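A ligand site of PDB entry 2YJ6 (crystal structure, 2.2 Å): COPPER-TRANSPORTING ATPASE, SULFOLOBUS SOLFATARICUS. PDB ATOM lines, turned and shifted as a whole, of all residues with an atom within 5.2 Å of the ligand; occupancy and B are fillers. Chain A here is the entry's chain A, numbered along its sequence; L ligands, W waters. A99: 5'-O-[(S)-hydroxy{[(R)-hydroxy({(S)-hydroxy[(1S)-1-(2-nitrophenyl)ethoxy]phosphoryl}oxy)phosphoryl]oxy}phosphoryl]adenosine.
NE2 of His 68 sits at hydrogen-bond distance from O3A of the ligand. The side-chain carboxylate (OE2) of Glu 63 sits at hydrogen-bond distance from a nitrogen (N1) of the ligand, at 2.7 Å.
OD1 of Asp 135 lies within hydrogen-bond range of N of Thr 43 (3.0 Å). The backbone NH (N) of Gly 42 sits at hydrogen-bond distance from the side-chain carboxylate (OD1) of Asp 135 (3.1 Å). The backbone NH (N) of Ile 70 lies within hydrogen-bond range of a ring nitrogen (ND1) of His 68 (2.8 Å). The backbone carbonyl oxygen (O) of Val 110 is in hydrogen-bond range of the backbone NH (N) of Val 99, at 3.2 Å. N of Ile 133 lies within hydrogen-bond range of OD2 of Asp 118 (2.8 Å).
The backbone carbonyl oxygen of Ile 97 sits close to an oxygen (O4') of the ligand. CG2 of Thr 36 touches C6' of the ligand, at 3.6 Å. O of Gly 42 touches C6' of the ligand (3.2 Å). N of Thr 43 touches C6' of the ligand (3.9 Å). Pro 44 touches the ligand (CD to C6', 3.7 Å). Ile 70 touches the ligand. Gly 96 touches the ligand (O to C5B, 3.3 Å). Gly 98 touches the ligand (CA to C4, 3.8 Å). Val 110 touches the ligand (O to C2, 3.6 Å). Lys 111 touches the ligand. CB of Lys 112 touches O2' of the ligand, at 3.5 Å. Ile 119 touches the ligand. Ile 133 touches the ligand (CG2 to O'M, 3.995 Å). C of Ser 134 touches O'M of the ligand (3.8 Å). Asp 135 touches the ligand. Hydrophobic or aromatic side chains that line the ligand: Pro 44, His 68, Ile 70, Val 110, Ile 119 and Ile 133. Of the 25 residues printed, 17 come within 4 Å of the ligand.
Water W1 lies within hydrogen-bond range of an oxygen (O2') of the ligand (2.7 Å) and the backbone carbonyl oxygen (O) of Asp 118 (3.2 Å).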
ATOM      1  N   THR A  36     -10.481  26.130  24.215  1.00  0.00           N
ATOM      2  CA  THR A  36     -11.868  25.742  23.942  1.00  0.00           C
ATOM      3  C   THR A  36     -12.263  24.377  24.531  1.00  0.00           C
ATOM      4  O   THR A  36     -11.656  23.360  24.195  1.00  0.00           O
ATOM      5  CB  THR A  36     -12.129  25.668  22.426  1.00  0.00           C
ATOM      6  OG1 THR A  36     -11.589  26.838  21.789  1.00  0.00           O
ATOM      7  CG2 THR A  36     -13.609  25.528  22.123  1.00  0.00           C
ATOM      8  N   GLY A  42     -17.129  25.533  25.638  1.00  0.00           N
ATOM      9  CA  GLY A  42     -17.017  25.190  24.225  1.00  0.00           C
ATOM     10  C   GLY A  42     -18.354  25.333  23.516  1.00  0.00           C
ATOM     11  O   GLY A  42     -18.636  24.598  22.563  1.00  0.00           O
ATOM     12  N   THR A  43     -19.177  26.275  23.971  1.00  0.00           N
ATOM     13  CA  THR A  43     -20.503  26.519  23.383  1.00  0.00           C
ATOM     14  C   THR A  43     -20.639  27.941  22.815  1.00  0.00           C
ATOM     15  O   THR A  43     -20.724  28.910  23.569  1.00  0.00           O
ATOM     16  CB  THR A  43     -21.622  26.327  24.419  1.00  0.00           C
ATOM     17  OG1 THR A  43     -21.466  27.285  25.467  1.00  0.00           O
ATOM     18  CG2 THR A  43     -21.583  24.931  25.003  1.00  0.00           C
ATOM     19  N   PRO A  44     -20.678  28.064  21.481  1.00  0.00           N
ATOM     20  CA  PRO A  44     -20.792  29.389  20.849  1.00  0.00           C
ATOM     21  C   PRO A  44     -22.141  30.107  21.038  1.00  0.00           C
ATOM     22  O   PRO A  44     -23.198  29.476  21.068  1.00  0.00           O
ATOM     23  CB  PRO A  44     -20.536  29.086  19.368  1.00  0.00           C
ATOM     24  CG  PRO A  44     -20.848  27.633  19.212  1.00  0.00           C
ATOM     25  CD  PRO A  44     -20.446  26.990  20.508  1.00  0.00           C
ATOM     26  N   GLU A  63     -28.892  28.071   7.576  1.00  0.00           N
ATOM     27  CA  GLU A  63     -28.126  27.432   8.641  1.00  0.00           C
ATOM     28  C   GLU A  63     -28.881  26.279   9.325  1.00  0.00           C
ATOM     29  O   GLU A  63     -28.271  25.406   9.936  1.00  0.00           O
ATOM     30  CB  GLU A  63     -27.704  28.466   9.675  1.00  0.00           C
ATOM     31  CG  GLU A  63     -26.711  29.496   9.163  1.00  0.00           C
ATOM     32  CD  GLU A  63     -25.290  28.952   9.094  1.00  0.00           C
ATOM     33  OE1 GLU A  63     -25.136  27.716   8.939  1.00  0.00           O
ATOM     34  OE2 GLU A  63     -24.351  29.749   9.212  1.00  0.00           O
ATOM     35  N   SER A  66     -27.814  22.674   8.758  1.00  0.00           N
ATOM     36  CA  SER A  66     -26.504  22.203   9.198  1.00  0.00           C
ATOM     37  C   SER A  66     -26.481  21.805  10.657  1.00  0.00           C
ATOM     38  O   SER A  66     -27.394  22.138  11.423  1.00  0.00           O
ATOM     39  CB  SER A  66     -25.423  23.237   8.962  1.00  0.00           C
ATOM     40  OG  SER A  66     -25.418  23.644   7.615  1.00  0.00           O
ATOM     41  N   HIS A  68     -23.367  22.100  12.259  1.00  0.00           N
ATOM     42  CA  HIS A  68     -22.251  22.845  12.812  1.00  0.00           C
ATOM     43  C   HIS A  68     -22.732  23.592  14.053  1.00  0.00           C
ATOM     44  O   HIS A  68     -23.878  24.078  14.106  1.00  0.00           O
ATOM     45  CB  HIS A  68     -21.676  23.814  11.790  1.00  0.00           C
ATOM     46  CG  HIS A  68     -20.302  24.306  12.133  1.00  0.00           C
ATOM     47  ND1 HIS A  68     -20.062  25.169  13.184  1.00  0.00           N
ATOM     48  CD2 HIS A  68     -19.100  24.050  11.571  1.00  0.00           C
ATOM     49  CE1 HIS A  68     -18.768  25.419  13.252  1.00  0.00           C
ATOM     50  NE2 HIS A  68     -18.157  24.760  12.282  1.00  0.00           N
ATOM     51  N   PRO A  69     -21.870  23.673  15.073  1.00  0.00           N
ATOM     52  CA  PRO A  69     -22.169  24.486  16.266  1.00  0.00           C
ATOM     53  C   PRO A  69     -22.470  25.959  15.917  1.00  0.00           C
ATOM     54  O   PRO A  69     -23.285  26.566  16.599  1.00  0.00           O
ATOM     55  CB  PRO A  69     -20.891  24.351  17.089  1.00  0.00           C
ATOM     56  CG  PRO A  69     -20.352  23.006  16.701  1.00  0.00           C
ATOM     57  CD  PRO A  69     -20.636  22.884  15.240  1.00  0.00           C
ATOM     58  N   ILE A  70     -21.827  26.504  14.886  1.00  0.00           N
ATOM     59  CA  ILE A  70     -22.136  27.862  14.435  1.00  0.00           C
ATOM     60  C   ILE A  70     -23.590  27.956  13.967  1.00  0.00           C
ATOM     61  O   ILE A  70     -24.337  28.841  14.367  1.00  0.00           O
ATOM     62  CB  ILE A  70     -21.254  28.330  13.270  1.00  0.00           C
ATOM     63  CG1 ILE A  70     -19.770  28.286  13.632  1.00  0.00           C
ATOM     64  CG2 ILE A  70     -21.674  29.750  12.819  1.00  0.00           C
ATOM     65  CD1 ILE A  70     -19.490  28.602  15.069  1.00  0.00           C
ATOM     66  N   ALA A  71     -23.963  27.020  13.100  1.00  0.00           N
ATOM     67  CA  ALA A  71     -25.306  26.993  12.549  1.00  0.00           C
ATOM     68  C   ALA A  71     -26.352  27.020  13.653  1.00  0.00           C
ATOM     69  O   ALA A  71     -27.280  27.831  13.625  1.00  0.00           O
ATOM     70  CB  ALA A  71     -25.475  25.754  11.681  1.00  0.00           C
ATOM     71  N   GLU A  93     -23.084  22.709   2.090  1.00  0.00           N
ATOM     72  CA  GLU A  93     -22.201  23.084   3.169  1.00  0.00           C
ATOM     73  C   GLU A  93     -20.791  22.718   2.773  1.00  0.00           C
ATOM     74  O   GLU A  93     -20.338  21.594   2.990  1.00  0.00           O
ATOM     75  CB  GLU A  93     -22.602  22.368   4.471  1.00  0.00           C
ATOM     76  CG  GLU A  93     -21.813  22.818   5.691  1.00  0.00           C
ATOM     77  CD  GLU A  93     -22.340  22.216   6.991  1.00  0.00           C
ATOM     78  OE1 GLU A  93     -23.481  21.698   6.990  1.00  0.00           O
ATOM     79  OE2 GLU A  93     -21.607  22.276   8.013  1.00  0.00           O
ATOM     80  N   GLY A  96     -15.498  23.314   6.179  1.00  0.00           N
ATOM     81  CA  GLY A  96     -14.331  24.123   6.471  1.00  0.00           C
ATOM     82  C   GLY A  96     -14.403  25.580   6.036  1.00  0.00           C
ATOM     83  O   GLY A  96     -13.440  26.325   6.225  1.00  0.00           O
ATOM     84  N   ILE A  97     -15.522  26.008   5.455  1.00  0.00           N
ATOM     85  CA  ILE A  97     -15.638  27.407   5.042  1.00  0.00           C
ATOM     86  C   ILE A  97     -16.978  28.065   5.437  1.00  0.00           C
ATOM     87  O   ILE A  97     -17.004  29.066   6.155  1.00  0.00           O
ATOM     88  CB  ILE A  97     -15.364  27.603   3.523  1.00  0.00           C
ATOM     89  CG1 ILE A  97     -16.469  26.961   2.684  1.00  0.00           C
ATOM     90  CG2 ILE A  97     -14.008  27.035   3.137  1.00  0.00           C
ATOM     91  N   GLY A  98     -18.078  27.498   4.952  1.00  0.00           N
ATOM     92  CA  GLY A  98     -19.391  28.051   5.206  1.00  0.00           C
ATOM     93  C   GLY A  98     -20.481  27.213   4.581  1.00  0.00           C
ATOM     94  O   GLY A  98     -20.301  26.008   4.356  1.00  0.00           O
ATOM     95  N   VAL A  99     -21.600  27.852   4.280  1.00  0.00           N
ATOM     96  CA  VAL A  99     -22.780  27.168   3.842  1.00  0.00           C
ATOM     97  C   VAL A  99     -23.495  27.977   2.767  1.00  0.00           C
ATOM     98  O   VAL A  99     -23.192  29.162   2.589  1.00  0.00           O
ATOM     99  CB  VAL A  99     -23.727  26.965   5.026  1.00  0.00           C
ATOM    100  CG1 VAL A  99     -24.480  28.278   5.349  1.00  0.00           C
ATOM    101  CG2 VAL A  99     -24.691  25.854   4.733  1.00  0.00           C
ATOM    102  N   VAL A 110     -23.316  32.164   3.801  1.00  0.00           N
ATOM    103  CA  VAL A 110     -22.893  32.557   5.147  1.00  0.00           C
ATOM    104  C   VAL A 110     -21.501  32.019   5.421  1.00  0.00           C
ATOM    105  O   VAL A 110     -21.295  30.805   5.336  1.00  0.00           O
ATOM    106  CB  VAL A 110     -23.825  31.965   6.236  1.00  0.00           C
ATOM    107  CG1 VAL A 110     -23.473  32.532   7.595  1.00  0.00           C
ATOM    108  CG2 VAL A 110     -25.305  32.184   5.915  1.00  0.00           C
ATOM    109  N   LYS A 111     -20.527  32.866   5.765  1.00  0.00           N
ATOM    110  CA  LYS A 111     -19.164  32.388   6.046  1.00  0.00           C
ATOM    111  C   LYS A 111     -18.279  33.317   6.899  1.00  0.00           C
ATOM    112  O   LYS A 111     -18.749  34.331   7.393  1.00  0.00           O
ATOM    113  CB  LYS A 111     -18.440  32.045   4.735  1.00  0.00           C
ATOM    114  CG  LYS A 111     -18.247  33.235   3.813  1.00  0.00           C
ATOM    115  CD  LYS A 111     -18.062  32.775   2.371  1.00  0.00           C
ATOM    116  CE  LYS A 111     -18.880  33.649   1.431  1.00  0.00           C
ATOM    117  NZ  LYS A 111     -20.259  33.852   2.002  1.00  0.00           N
ATOM    118  N   LYS A 112     -16.999  32.959   7.052  1.00  0.00           N
ATOM    119  CA  LYS A 112     -16.060  33.773   7.837  1.00  0.00           C
ATOM    120  C   LYS A 112     -15.924  35.192   7.278  1.00  0.00           C
ATOM    121  O   LYS A 112     -15.806  35.374   6.063  1.00  0.00           O
ATOM    122  CB  LYS A 112     -14.682  33.110   7.894  1.00  0.00           C
ATOM    123  N   ASP A 118     -16.973  38.294  12.822  1.00  0.00           N
ATOM    124  CA  ASP A 118     -16.650  36.880  12.710  1.00  0.00           C
ATOM    125  C   ASP A 118     -17.326  36.256  11.481  1.00  0.00           C
ATOM    126  O   ASP A 118     -16.681  35.550  10.710  1.00  0.00           O
ATOM    127  CB  ASP A 118     -17.076  36.130  13.983  1.00  0.00           C
ATOM    128  CG  ASP A 118     -16.388  36.662  15.245  1.00  0.00           C
ATOM    129  OD1 ASP A 118     -15.154  36.846  15.250  1.00  0.00           O
ATOM    130  OD2 ASP A 118     -17.097  36.884  16.252  1.00  0.00           O
ATOM    131  N   ILE A 119     -18.622  36.532  11.288  1.00  0.00           N
ATOM    132  CA  ILE A 119     -19.405  35.876  10.242  1.00  0.00           C
ATOM    133  C   ILE A 119     -20.127  36.874   9.307  1.00  0.00           C
ATOM    134  O   ILE A 119     -20.599  37.912   9.752  1.00  0.00           O
ATOM    135  CB  ILE A 119     -20.459  34.928  10.866  1.00  0.00           C
ATOM    136  CG1 ILE A 119     -19.784  33.878  11.768  1.00  0.00           C
ATOM    137  CG2 ILE A 119     -21.324  34.274   9.780  1.00  0.00           C
ATOM    138  CD1 ILE A 119     -18.758  33.012  11.045  1.00  0.00           C
ATOM    139  N   ILE A 133     -19.660  36.243  17.263  1.00  0.00           N
ATOM    140  CA  ILE A 133     -19.935  34.999  17.974  1.00  0.00           C
ATOM    141  C   ILE A 133     -18.879  34.742  19.045  1.00  0.00           C
ATOM    142  O   ILE A 133     -17.695  34.938  18.793  1.00  0.00           O
ATOM    143  CB  ILE A 133     -19.966  33.841  16.970  1.00  0.00           C
ATOM    144  CG1 ILE A 133     -21.206  33.960  16.091  1.00  0.00           C
ATOM    145  CG2 ILE A 133     -19.932  32.504  17.679  1.00  0.00           C
ATOM    146  CD1 ILE A 133     -21.298  32.925  15.022  1.00  0.00           C
ATOM    147  N   SER A 134     -19.327  34.311  20.224  1.00  0.00           N
ATOM    148  CA  SER A 134     -18.421  34.036  21.357  1.00  0.00           C
ATOM    149  C   SER A 134     -18.700  32.723  22.091  1.00  0.00           C
ATOM    150  O   SER A 134     -19.748  32.101  21.907  1.00  0.00           O
ATOM    151  CB  SER A 134     -18.473  35.178  22.381  1.00  0.00           C
ATOM    152  OG  SER A 134     -18.050  36.397  21.793  1.00  0.00           O
ATOM    153  N   ASP A 135     -17.736  32.317  22.920  1.00  0.00           N
ATOM    154  CA  ASP A 135     -17.811  31.135  23.778  1.00  0.00           C
ATOM    155  C   ASP A 135     -18.172  31.664  25.164  1.00  0.00           C
ATOM    156  O   ASP A 135     -18.203  32.887  25.360  1.00  0.00           O
ATOM    157  CB  ASP A 135     -16.421  30.464  23.826  1.00  0.00           C
ATOM    158  CG  ASP A 135     -16.474  28.967  24.149  1.00  0.00           C
ATOM    159  OD1 ASP A 135     -17.391  28.506  24.852  1.00  0.00           O
ATOM    160  OD2 ASP A 135     -15.567  28.241  23.665  1.00  0.00           O
ATOM    161  N   ASP A 161      -7.977  31.247  18.591  1.00  0.00           N
ATOM    162  CA  ASP A 161      -8.623  32.563  18.469  1.00  0.00           C
ATOM    163  C   ASP A 161      -7.651  33.732  18.375  1.00  0.00           C
ATOM    164  O   ASP A 161      -6.443  33.566  18.514  1.00  0.00           O
ATOM    165  CB  ASP A 161      -9.587  32.790  19.639  1.00  0.00           C
ATOM    166  CG  ASP A 161     -10.762  31.824  19.640  1.00  0.00           C
ATOM    167  OD1 ASP A 161     -10.948  31.105  18.628  1.00  0.00           O
ATOM    168  OD2 ASP A 161     -11.494  31.787  20.641  1.00  0.00           O
ATOM    169  N   ASN A 209      -9.055  19.579  17.490  1.00  0.00           N
ATOM    170  CA  ASN A 209      -7.744  20.013  17.023  1.00  0.00           C
ATOM    171  C   ASN A 209      -6.690  19.888  18.108  1.00  0.00           C
ATOM    172  O   ASN A 209      -5.872  20.788  18.300  1.00  0.00           O
ATOM    173  CB  ASN A 209      -7.802  21.460  16.512  1.00  0.00           C
ATOM    174  CG  ASN A 209      -8.609  21.609  15.237  1.00  0.00           C
ATOM    175  OD1 ASN A 209      -9.275  22.619  15.020  1.00  0.00           O
ATOM    176  ND2 ASN A 209      -8.578  20.570  14.399  1.00  0.00           N
HETATM  177  C'  A99 L   1     -16.641  27.398  16.675  1.00  0.00           C
HETATM  178  N1  A99 L   1     -21.878  28.758   8.846  1.00  0.00           N
HETATM  179  C2  A99 L   1     -21.138  29.885   8.832  1.00  0.00           C
HETATM  180  N3  A99 L   1     -19.805  29.875   8.895  1.00  0.00           N
HETATM  181  C4  A99 L   1     -19.116  28.709   8.966  1.00  0.00           C
HETATM  182  C5  A99 L   1     -19.863  27.434   8.990  1.00  0.00           C
HETATM  183  C6  A99 L   1     -21.336  27.519   8.920  1.00  0.00           C
HETATM  184  N6  A99 L   1     -22.117  26.403   8.933  1.00  0.00           N
HETATM  185  N7  A99 L   1     -18.946  26.454   9.065  1.00  0.00           N
HETATM  186  C8  A99 L   1     -17.726  27.044   9.105  1.00  0.00           C
HETATM  187  N9  A99 L   1     -17.828  28.383   9.043  1.00  0.00           N
HETATM  188  PA  A99 L   1     -13.987  25.114  10.881  1.00  0.00           P
HETATM  189  PB  A99 L   1     -14.353  25.265  13.656  1.00  0.00           P
HETATM  190  PG  A99 L   1     -14.150  27.307  15.604  1.00  0.00           P
HETATM  191  O'L A99 L   1     -16.189  29.960  17.716  1.00  0.00           O
HETATM  192  O'M A99 L   1     -17.084  30.446  19.580  1.00  0.00           O
HETATM  193  C1' A99 L   1     -16.746  27.926  20.490  1.00  0.00           C
HETATM  194  O1A A99 L   1     -12.567  25.469  11.234  1.00  0.00           O
HETATM  195  C1B A99 L   1     -16.697  29.339   9.045  1.00  0.00           C
HETATM  196  O1B A99 L   1     -15.234  24.237  14.341  1.00  0.00           O
HETATM  197  O1G A99 L   1     -13.757  26.145  16.494  1.00  0.00           O
HETATM  198  C2' A99 L   1     -16.689  28.258  19.152  1.00  0.00           C
HETATM  199  N2' A99 L   1     -16.648  29.609  18.794  1.00  0.00           N
HETATM  200  O2' A99 L   1     -15.987  31.094  10.500  1.00  0.00           O
HETATM  201  O2A A99 L   1     -14.322  23.740  10.343  1.00  0.00           O
HETATM  202  C2B A99 L   1     -16.342  29.712  10.460  1.00  0.00           C
HETATM  203  O2B A99 L   1     -12.848  25.092  13.636  1.00  0.00           O
HETATM  204  O2G A99 L   1     -15.426  28.060  16.248  1.00  0.00           O
HETATM  205  C3' A99 L   1     -16.677  27.166  18.138  1.00  0.00           C
HETATM  206  O3' A99 L   1     -14.282  29.525  11.718  1.00  0.00           O
HETATM  207  O3A A99 L   1     -14.917  25.385  12.152  1.00  0.00           O
HETATM  208  C3B A99 L   1     -15.143  28.843  10.801  1.00  0.00           C
HETATM  209  O3B A99 L   1     -14.722  26.740  14.209  1.00  0.00           O
HETATM  210  O3G A99 L   1     -13.103  28.355  15.282  1.00  0.00           O
HETATM  211  C4' A99 L   1     -16.744  25.851  18.585  1.00  0.00           C
HETATM  212  O4' A99 L   1     -15.542  28.689   8.474  1.00  0.00           O
HETATM  213  C4B A99 L   1     -14.499  28.597   9.444  1.00  0.00           C
HETATM  214  C5' A99 L   1     -16.793  25.566  19.941  1.00  0.00           C
HETATM  215  O5' A99 L   1     -14.594  26.223   9.887  1.00  0.00           O
HETATM  216  C5B A99 L   1     -13.775  27.258   9.357  1.00  0.00           C
HETATM  217  C6' A99 L   1     -16.797  26.596  20.884  1.00  0.00           C
HETATM  218  CM' A99 L   1     -16.869  26.074  15.959  1.00  0.00           C
HETATM  219  O   HOH W   1     -15.153  33.108  12.108  1.00  0.00           O
